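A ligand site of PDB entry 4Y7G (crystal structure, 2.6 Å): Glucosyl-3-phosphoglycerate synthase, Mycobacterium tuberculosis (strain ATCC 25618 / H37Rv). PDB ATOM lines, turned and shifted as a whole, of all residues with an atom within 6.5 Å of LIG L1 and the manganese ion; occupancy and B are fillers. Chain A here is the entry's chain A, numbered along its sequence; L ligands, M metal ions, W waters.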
ATOM      1  N   GLU A  58      20.158  18.766 -20.339  1.00  0.00           N
ATOM      2  CA  GLU A  58      19.490  19.888 -21.002  1.00  0.00           C
ATOM      3  C   GLU A  58      17.949  19.769 -20.972  1.00  0.00           C
ATOM      4  O   GLU A  58      17.286  20.089 -21.962  1.00  0.00           O
ATOM      5  CB  GLU A  58      20.000  19.996 -22.445  1.00  0.00           C
ATOM      6  CG  GLU A  58      21.532  20.048 -22.571  1.00  0.00           C
ATOM      7  CD  GLU A  58      22.167  21.301 -21.969  1.00  0.00           C
ATOM      8  OE1 GLU A  58      21.480  22.054 -21.258  1.00  0.00           O
ATOM      9  OE2 GLU A  58      23.364  21.548 -22.195  1.00  0.00           O
ATOM     10  N   ASP A 138      23.291  21.565 -31.057  1.00  0.00           N
ATOM     11  CA  ASP A 138      23.342  21.491 -29.606  1.00  0.00           C
ATOM     12  C   ASP A 138      21.933  21.471 -29.050  1.00  0.00           C
ATOM     13  O   ASP A 138      21.027  22.100 -29.590  1.00  0.00           O
ATOM     14  CB  ASP A 138      24.083  22.675 -28.987  1.00  0.00           C
ATOM     15  CG  ASP A 138      25.602  22.620 -29.193  1.00  0.00           C
ATOM     16  OD1 ASP A 138      26.200  21.546 -29.443  1.00  0.00           O
ATOM     17  OD2 ASP A 138      26.209  23.722 -29.095  1.00  0.00           O
ATOM     18  N   ASP A 140      21.113  22.552 -26.057  1.00  0.00           N
ATOM     19  CA  ASP A 140      20.928  23.642 -25.093  1.00  0.00           C
ATOM     20  C   ASP A 140      20.515  24.958 -25.744  1.00  0.00           C
ATOM     21  O   ASP A 140      20.485  26.009 -25.087  1.00  0.00           O
ATOM     22  CB  ASP A 140      22.217  23.876 -24.298  1.00  0.00           C
ATOM     23  CG  ASP A 140      23.256  24.644 -25.090  1.00  0.00           C
ATOM     24  OD1 ASP A 140      23.408  24.378 -26.310  1.00  0.00           O
ATOM     25  OD2 ASP A 140      23.946  25.498 -24.494  1.00  0.00           O
ATOM     26  N   LEU A 141      20.150  24.911 -27.025  1.00  0.00           N
ATOM     27  CA  LEU A 141      19.744  26.118 -27.740  1.00  0.00           C
ATOM     28  C   LEU A 141      18.398  26.643 -27.267  1.00  0.00           C
ATOM     29  O   LEU A 141      17.477  25.892 -27.032  1.00  0.00           O
ATOM     30  CB  LEU A 141      19.713  25.837 -29.243  1.00  0.00           C
ATOM     31  CG  LEU A 141      21.046  25.403 -29.800  1.00  0.00           C
ATOM     32  CD1 LEU A 141      20.861  25.048 -31.250  1.00  0.00           C
ATOM     33  CD2 LEU A 141      22.107  26.494 -29.629  1.00  0.00           C
ATOM     34  N   GLY A 188      30.556  34.818 -27.701  1.00  0.00           N
ATOM     35  CA  GLY A 188      31.674  33.958 -28.036  1.00  0.00           C
ATOM     36  C   GLY A 188      32.937  34.298 -27.293  1.00  0.00           C
ATOM     37  O   GLY A 188      33.944  34.626 -27.908  1.00  0.00           O
ATOM     38  N   ARG A 189      32.902  34.258 -25.958  1.00  0.00           N
ATOM     39  CA  ARG A 189      34.102  34.535 -25.191  1.00  0.00           C
ATOM     40  C   ARG A 189      35.284  33.573 -25.478  1.00  0.00           C
ATOM     41  O   ARG A 189      36.424  34.016 -25.641  1.00  0.00           O
ATOM     42  CB  ARG A 189      33.779  34.482 -23.710  1.00  0.00           C
ATOM     43  CG  ARG A 189      33.439  35.812 -23.099  1.00  0.00           C
ATOM     44  CD  ARG A 189      32.836  35.619 -21.695  1.00  0.00           C
ATOM     45  NE  ARG A 189      31.670  34.718 -21.712  1.00  0.00           N
ATOM     46  CZ  ARG A 189      31.016  34.304 -20.620  1.00  0.00           C
ATOM     47  NH1 ARG A 189      31.422  34.728 -19.418  1.00  0.00           N
ATOM     48  NH2 ARG A 189      29.982  33.483 -20.721  1.00  0.00           N
ATOM     49  N   VAL A 190      35.019  32.271 -25.479  1.00  0.00           N
ATOM     50  CA  VAL A 190      36.089  31.317 -25.748  1.00  0.00           C
ATOM     51  C   VAL A 190      36.471  31.491 -27.201  1.00  0.00           C
ATOM     52  O   VAL A 190      37.655  31.444 -27.569  1.00  0.00           O
ATOM     53  CB  VAL A 190      35.695  29.866 -25.422  1.00  0.00           C
ATOM     54  CG1 VAL A 190      36.718  28.892 -26.000  1.00  0.00           C
ATOM     55  CG2 VAL A 190      35.594  29.708 -23.898  1.00  0.00           C
ATOM     56  N   THR A 191      35.452  31.665 -28.027  1.00  0.00           N
ATOM     57  CA  THR A 191      35.594  31.807 -29.471  1.00  0.00           C
ATOM     58  C   THR A 191      36.436  33.037 -29.796  1.00  0.00           C
ATOM     59  O   THR A 191      37.338  32.970 -30.627  1.00  0.00           O
ATOM     60  CB  THR A 191      34.234  31.891 -30.172  1.00  0.00           C
ATOM     61  OG1 THR A 191      33.540  30.657 -29.976  1.00  0.00           O
ATOM     62  CG2 THR A 191      34.388  32.125 -31.676  1.00  0.00           C
ATOM     63  N   GLU A 192      36.086  34.168 -29.201  1.00  0.00           N
ATOM     64  CA  GLU A 192      36.713  35.411 -29.600  1.00  0.00           C
ATOM     65  C   GLU A 192      38.046  35.661 -28.917  1.00  0.00           C
ATOM     66  O   GLU A 192      38.891  36.360 -29.457  1.00  0.00           O
ATOM     67  CB  GLU A 192      35.772  36.593 -29.336  1.00  0.00           C
ATOM     68  CG  GLU A 192      34.506  36.616 -30.184  1.00  0.00           C
ATOM     69  CD  GLU A 192      34.763  36.594 -31.687  1.00  0.00           C
ATOM     70  OE1 GLU A 192      35.905  36.833 -32.148  1.00  0.00           O
ATOM     71  OE2 GLU A 192      33.810  36.319 -32.434  1.00  0.00           O
ATOM     72  N   GLN A 211      32.771  31.340 -36.705  1.00  0.00           N
ATOM     73  CA  GLN A 211      32.376  30.610 -35.497  1.00  0.00           C
ATOM     74  C   GLN A 211      32.941  29.195 -35.533  1.00  0.00           C
ATOM     75  O   GLN A 211      32.212  28.230 -35.711  1.00  0.00           O
ATOM     76  CB  GLN A 211      30.840  30.553 -35.348  1.00  0.00           C
ATOM     77  CG  GLN A 211      30.117  31.898 -35.348  1.00  0.00           C
ATOM     78  CD  GLN A 211      30.551  32.806 -34.228  1.00  0.00           C
ATOM     79  OE1 GLN A 211      31.055  32.349 -33.196  1.00  0.00           O
ATOM     80  NE2 GLN A 211      30.340  34.107 -34.411  1.00  0.00           N
ATOM     81  N   LEU A 213      34.020  27.339 -33.282  1.00  0.00           N
ATOM     82  CA  LEU A 213      33.543  26.519 -32.164  1.00  0.00           C
ATOM     83  C   LEU A 213      32.049  26.210 -32.252  1.00  0.00           C
ATOM     84  O   LEU A 213      31.491  25.603 -31.350  1.00  0.00           O
ATOM     85  CB  LEU A 213      33.862  27.197 -30.823  1.00  0.00           C
ATOM     86  CG  LEU A 213      35.354  27.424 -30.537  1.00  0.00           C
ATOM     87  CD1 LEU A 213      35.541  27.835 -29.100  1.00  0.00           C
ATOM     88  CD2 LEU A 213      36.276  26.196 -30.889  1.00  0.00           C
ATOM     89  N   SER A 214      31.397  26.606 -33.337  1.00  0.00           N
ATOM     90  CA  SER A 214      29.960  26.411 -33.390  1.00  0.00           C
ATOM     91  C   SER A 214      29.529  24.959 -33.242  1.00  0.00           C
ATOM     92  O   SER A 214      30.089  24.058 -33.886  1.00  0.00           O
ATOM     93  CB  SER A 214      29.418  26.933 -34.709  1.00  0.00           C
ATOM     94  OG  SER A 214      27.994  26.885 -34.651  1.00  0.00           O
ATOM     95  N   ARG A 260      21.978  33.614 -31.939  1.00  0.00           N
ATOM     96  CA  ARG A 260      21.949  32.454 -31.068  1.00  0.00           C
ATOM     97  C   ARG A 260      22.009  32.758 -29.608  1.00  0.00           C
ATOM     98  O   ARG A 260      22.702  33.652 -29.134  1.00  0.00           O
ATOM     99  CB  ARG A 260      23.193  31.644 -31.383  1.00  0.00           C
ATOM    100  CG  ARG A 260      23.271  30.213 -30.928  1.00  0.00           C
ATOM    101  CD  ARG A 260      24.728  29.886 -30.596  1.00  0.00           C
ATOM    102  NE  ARG A 260      25.000  28.444 -30.534  1.00  0.00           N
ATOM    103  CZ  ARG A 260      25.998  27.891 -29.842  1.00  0.00           C
ATOM    104  NH1 ARG A 260      26.148  26.569 -29.865  1.00  0.00           N
ATOM    105  NH2 ARG A 260      26.833  28.651 -29.141  1.00  0.00           N
ATOM    106  N   HIS A 262      22.001  30.499 -25.796  1.00  0.00           N
ATOM    107  CA  HIS A 262      22.150  29.180 -25.197  1.00  0.00           C
ATOM    108  C   HIS A 262      22.486  29.382 -23.743  1.00  0.00           C
ATOM    109  O   HIS A 262      22.611  30.517 -23.284  1.00  0.00           O
ATOM    110  CB  HIS A 262      23.184  28.316 -25.939  1.00  0.00           C
ATOM    111  CG  HIS A 262      24.577  28.823 -25.857  1.00  0.00           C
ATOM    112  ND1 HIS A 262      25.665  28.009 -25.605  1.00  0.00           N
ATOM    113  CD2 HIS A 262      25.075  30.072 -26.011  1.00  0.00           C
ATOM    114  CE1 HIS A 262      26.770  28.732 -25.605  1.00  0.00           C
ATOM    115  NE2 HIS A 262      26.434  29.993 -25.843  1.00  0.00           N
ATOM    116  N   ARG A 263      22.651  28.267 -23.045  1.00  0.00           N
ATOM    117  CA  ARG A 263      23.070  28.306 -21.639  1.00  0.00           C
ATOM    118  C   ARG A 263      24.363  29.091 -21.501  1.00  0.00           C
ATOM    119  O   ARG A 263      25.347  28.836 -22.194  1.00  0.00           O
ATOM    120  CB  ARG A 263      23.256  26.893 -21.112  1.00  0.00           C
ATOM    121  CG  ARG A 263      23.551  26.824 -19.624  1.00  0.00           C
ATOM    122  CD  ARG A 263      24.107  25.467 -19.254  1.00  0.00           C
ATOM    123  NE  ARG A 263      23.164  24.374 -19.514  1.00  0.00           N
ATOM    124  CZ  ARG A 263      22.278  23.932 -18.637  1.00  0.00           C
ATOM    125  NH1 ARG A 263      22.193  24.479 -17.434  1.00  0.00           N
ATOM    126  NH2 ARG A 263      21.489  22.929 -18.947  1.00  0.00           N
ATOM    127  N   ASN A 264      24.348  30.065 -20.590  1.00  0.00           N
ATOM    128  CA  ASN A 264      25.600  30.700 -20.201  1.00  0.00           C
ATOM    129  C   ASN A 264      26.242  30.137 -18.988  1.00  0.00           C
ATOM    130  O   ASN A 264      25.765  30.266 -17.866  1.00  0.00           O
ATOM    131  CB  ASN A 264      25.373  32.196 -19.946  1.00  0.00           C
ATOM    132  CG  ASN A 264      24.870  32.924 -21.174  1.00  0.00           C
ATOM    133  OD1 ASN A 264      25.369  32.725 -22.296  1.00  0.00           O
ATOM    134  ND2 ASN A 264      23.872  33.780 -20.974  1.00  0.00           N
ATOM    135  N   ARG A 265      27.320  29.423 -19.270  1.00  0.00           N
ATOM    136  CA  ARG A 265      28.145  28.764 -18.287  1.00  0.00           C
ATOM    137  C   ARG A 265      28.989  29.731 -17.453  1.00  0.00           C
ATOM    138  O   ARG A 265      29.334  30.826 -17.923  1.00  0.00           O
ATOM    139  CB  ARG A 265      28.980  27.729 -19.003  1.00  0.00           C
ATOM    140  CG  ARG A 265      28.109  26.810 -19.848  1.00  0.00           C
ATOM    141  CD  ARG A 265      28.953  25.893 -20.687  1.00  0.00           C
ATOM    142  NE  ARG A 265      29.668  24.932 -19.860  1.00  0.00           N
ATOM    143  CZ  ARG A 265      30.831  24.397 -20.180  1.00  0.00           C
ATOM    144  NH1 ARG A 265      31.446  24.720 -21.323  1.00  0.00           N
ATOM    145  NH2 ARG A 265      31.391  23.525 -19.340  1.00  0.00           N
ATOM    146  N   LEU A 270      34.293  27.581 -18.451  1.00  0.00           N
ATOM    147  CA  LEU A 270      34.825  28.043 -19.727  1.00  0.00           C
ATOM    148  C   LEU A 270      36.325  27.956 -19.726  1.00  0.00           C
ATOM    149  O   LEU A 270      36.936  27.749 -20.759  1.00  0.00           O
ATOM    150  CB  LEU A 270      34.398  29.487 -19.986  1.00  0.00           C
ATOM    151  CG  LEU A 270      32.904  29.768 -20.132  1.00  0.00           C
ATOM    152  CD1 LEU A 270      32.707  31.242 -20.389  1.00  0.00           C
ATOM    153  CD2 LEU A 270      32.273  28.925 -21.244  1.00  0.00           C
ATOM    154  N   MET A 273      37.108  24.621 -20.571  1.00  0.00           N
ATOM    155  CA  MET A 273      36.765  24.325 -21.951  1.00  0.00           C
ATOM    156  C   MET A 273      37.902  24.833 -22.827  1.00  0.00           C
ATOM    157  O   MET A 273      38.370  24.168 -23.739  1.00  0.00           O
ATOM    158  CB  MET A 273      35.448  24.971 -22.350  1.00  0.00           C
ATOM    159  CG  MET A 273      35.203  24.905 -23.830  1.00  0.00           C
ATOM    160  SD  MET A 273      33.522  25.273 -24.342  1.00  0.00           S
ATOM    161  CE  MET A 273      33.409  27.013 -24.091  1.00  0.00           C
HETATM  162  O1  LIG L   1      31.794  30.230 -27.751  1.00  0.00           O
HETATM  163  C1  LIG L   1      30.418  29.977 -27.999  1.00  0.00           C
HETATM  164  C2  LIG L   1      29.522  31.207 -27.778  1.00  0.00           C
HETATM  165  O2  LIG L   1      28.232  30.955 -28.317  1.00  0.00           O
HETATM  166  C3  LIG L   1      29.469  31.479 -26.255  1.00  0.00           C
HETATM  167  O3  LIG L   1      29.607  32.818 -25.804  1.00  0.00           O
HETATM  168  O4  LIG L   1      28.470  34.446 -24.135  1.00  0.00           O
HETATM  169  O5  LIG L   1      30.561  33.349 -23.480  1.00  0.00           O
HETATM  170  O6  LIG L   1      28.509  32.031 -23.594  1.00  0.00           O
HETATM  171  P1  LIG L   1      29.280  33.167 -24.243  1.00  0.00           P
HETATM  172  N1  LG2 L   2      27.498  18.017 -24.184  1.00  0.00           N
HETATM  173  C1  LG2 L   2      27.525  16.618 -24.087  1.00  0.00           C
HETATM  174  N2  LG2 L   2      28.443  16.013 -23.317  1.00  0.00           N
HETATM  175  C2  LG2 L   2      29.335  16.716 -22.610  1.00  0.00           C
HETATM  176  C3  LG2 L   2      29.326  18.104 -22.685  1.00  0.00           C
HETATM  177  C4  LG2 L   2      28.393  18.734 -23.490  1.00  0.00           C
HETATM  178  O1  LG2 L   2      26.700  15.942 -24.735  1.00  0.00           O
HETATM  179  O2  LG2 L   2      30.178  16.114 -21.897  1.00  0.00           O
HETATM  180  C5  LG2 L   2      26.495  18.672 -25.035  1.00  0.00           C
HETATM  181  C6  LG2 L   2      25.586  19.644 -24.268  1.00  0.00           C
HETATM  182  O3  LG2 L   2      24.367  19.057 -23.809  1.00  0.00           O
HETATM  183  C7  LG2 L   2      25.309  20.729 -25.270  1.00  0.00           C
HETATM  184  C8  LG2 L   2      26.448  20.632 -26.275  1.00  0.00           C
HETATM  185  O4  LG2 L   2      27.162  19.429 -26.020  1.00  0.00           O
HETATM  186  O5  LG2 L   2      24.092  20.485 -25.954  1.00  0.00           O
HETATM  187  C9  LG2 L   2      27.404  21.801 -26.156  1.00  0.00           C
HETATM  188  O6  LG2 L   2      27.856  21.838 -24.809  1.00  0.00           O
HETATM  189  P1  LG2 L   2      27.959  23.244 -24.070  1.00  0.00           P
HETATM  190  O7  LG2 L   2      26.659  23.993 -24.268  1.00  0.00           O
HETATM  191  O8  LG2 L   2      28.275  22.999 -22.612  1.00  0.00           O
HETATM  192  O9  LG2 L   2      29.160  23.951 -24.841  1.00  0.00           O
HETATM  193  P2  LG2 L   2      29.400  25.523 -25.087  1.00  0.00           P
HETATM  194  O10 LG2 L   2      29.860  26.268 -23.874  1.00  0.00           O
HETATM  195  O11 LG2 L   2      28.241  26.186 -25.805  1.00  0.00           O
HETATM  196  O12 LG2 L   2      30.649  25.386 -26.102  1.00  0.00           O
HETATM  197  C10 LG2 L   2      30.699  25.916 -27.422  1.00  0.00           C
HETATM  198  C11 LG2 L   2      29.778  25.159 -28.383  1.00  0.00           C
HETATM  199  C12 LG2 L   2      30.015  23.670 -28.181  1.00  0.00           C
HETATM  200  C13 LG2 L   2      31.475  23.396 -28.481  1.00  0.00           C
HETATM  201  C14 LG2 L   2      32.401  24.299 -27.659  1.00  0.00           C
HETATM  202  C15 LG2 L   2      33.860  24.085 -28.060  1.00  0.00           C
HETATM  203  O13 LG2 L   2      28.395  25.519 -28.183  1.00  0.00           O
HETATM  204  O14 LG2 L   2      29.178  22.921 -29.055  1.00  0.00           O
HETATM  205  O15 LG2 L   2      31.830  22.059 -28.188  1.00  0.00           O
HETATM  206  O16 LG2 L   2      32.023  25.673 -27.835  1.00  0.00           O
HETATM  207  O17 LG2 L   2      33.927  23.877 -29.475  1.00  0.00           O
HETATM  208 MN    MN M   1      26.064  25.988 -24.970  1.00  0.00          MN
HETATM  209  O   HOH W   1      28.484  29.373 -22.761  1.00  0.00           O
HETATM  210  O   HOH W   2      25.494  25.240 -26.933  1.00  0.00           O
HETATM  211  O   HOH W   3      26.650  26.350 -22.896  1.00  0.00           O
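Water W3 lies within hydrogen-bond range of the backbone carbonyl oxygen of Arg 263 (2.9 Å) and an oxygen (O10) of LG2 L2 (3.4 Å).
Water W2 lies within hydrogen-bond range of the side-chain carboxylate (OD2) of Asp 138 (2.7 Å), an oxygen (O13) of LG2 L2 (3.2 Å) and the guanidinium group (NH1) of Arg 260 (3.3 Å).
Water W1 lies within hydrogen-bond range of O6 of LIG L1 (2.8 Å) and O of Arg 263 (3.2 Å).
NH1 of Arg 260 is in salt-bridge range of OD2 of Asp 138, at 2.9 Å.
The side-chain carboxylate of Asp 140 sits close to the backbone NH of Arg 263 (3.4 Å).
The manganese ion is bound by a ring nitrogen (ND1) of His 262 (2.2 Å), water W2 (2.2 Å), water W3 (2.2 Å), an oxygen (O7) of LG2 L2 (2.2 Å), the side-chain carboxylate of Asp 140 (2.2 Å) and an oxygen (O11) of LG2 L2 (2.3 Å).
The manganese ion has six donor atoms within binding distance.
Of the 19 residues printed, 2 come within 4 Å of the manganese ion.
The side-chain carboxylate of Asp 138 is in hydrogen-bond range of an oxygen (O13) of LG2 L2.
OG1 of Thr 191 sits at hydrogen-bond distance from O1 of LIG L1 (2.9 Å).
An oxygen (O10) of LG2 L2 lies within salt-bridge range of the guanidinium group of Arg 265.
O2 of LIG L1 is in hydrogen-bond range of NH2 of Arg 260 (2.8 Å).
OD1 of Asn 264 sits close to O6 of LIG L1 (3.5 Å).
NE2 of His 262 sits at hydrogen-bond distance from O2 of LIG L1, 3.2 Å away.
The side-chain carboxylate (OE2) of Glu 58 lies within hydrogen-bond range of an oxygen (O3) of LG2 L2 (3.1 Å).
An oxygen (O5) of LIG L1 lies within salt-bridge range of the guanidinium group (NE) of Arg 189 (2.5 Å).
The backbone NH (N) of Gly 188 sits at hydrogen-bond distance from an oxygen (O3) of LIG L1 (2.9 Å).
The guanidinium group (NH1) of Arg 260 is in hydrogen-bond range of an oxygen (O13) of LG2 L2.
Hydrophobic or aromatic side chains within 4 Å of LIG L1: His 262.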
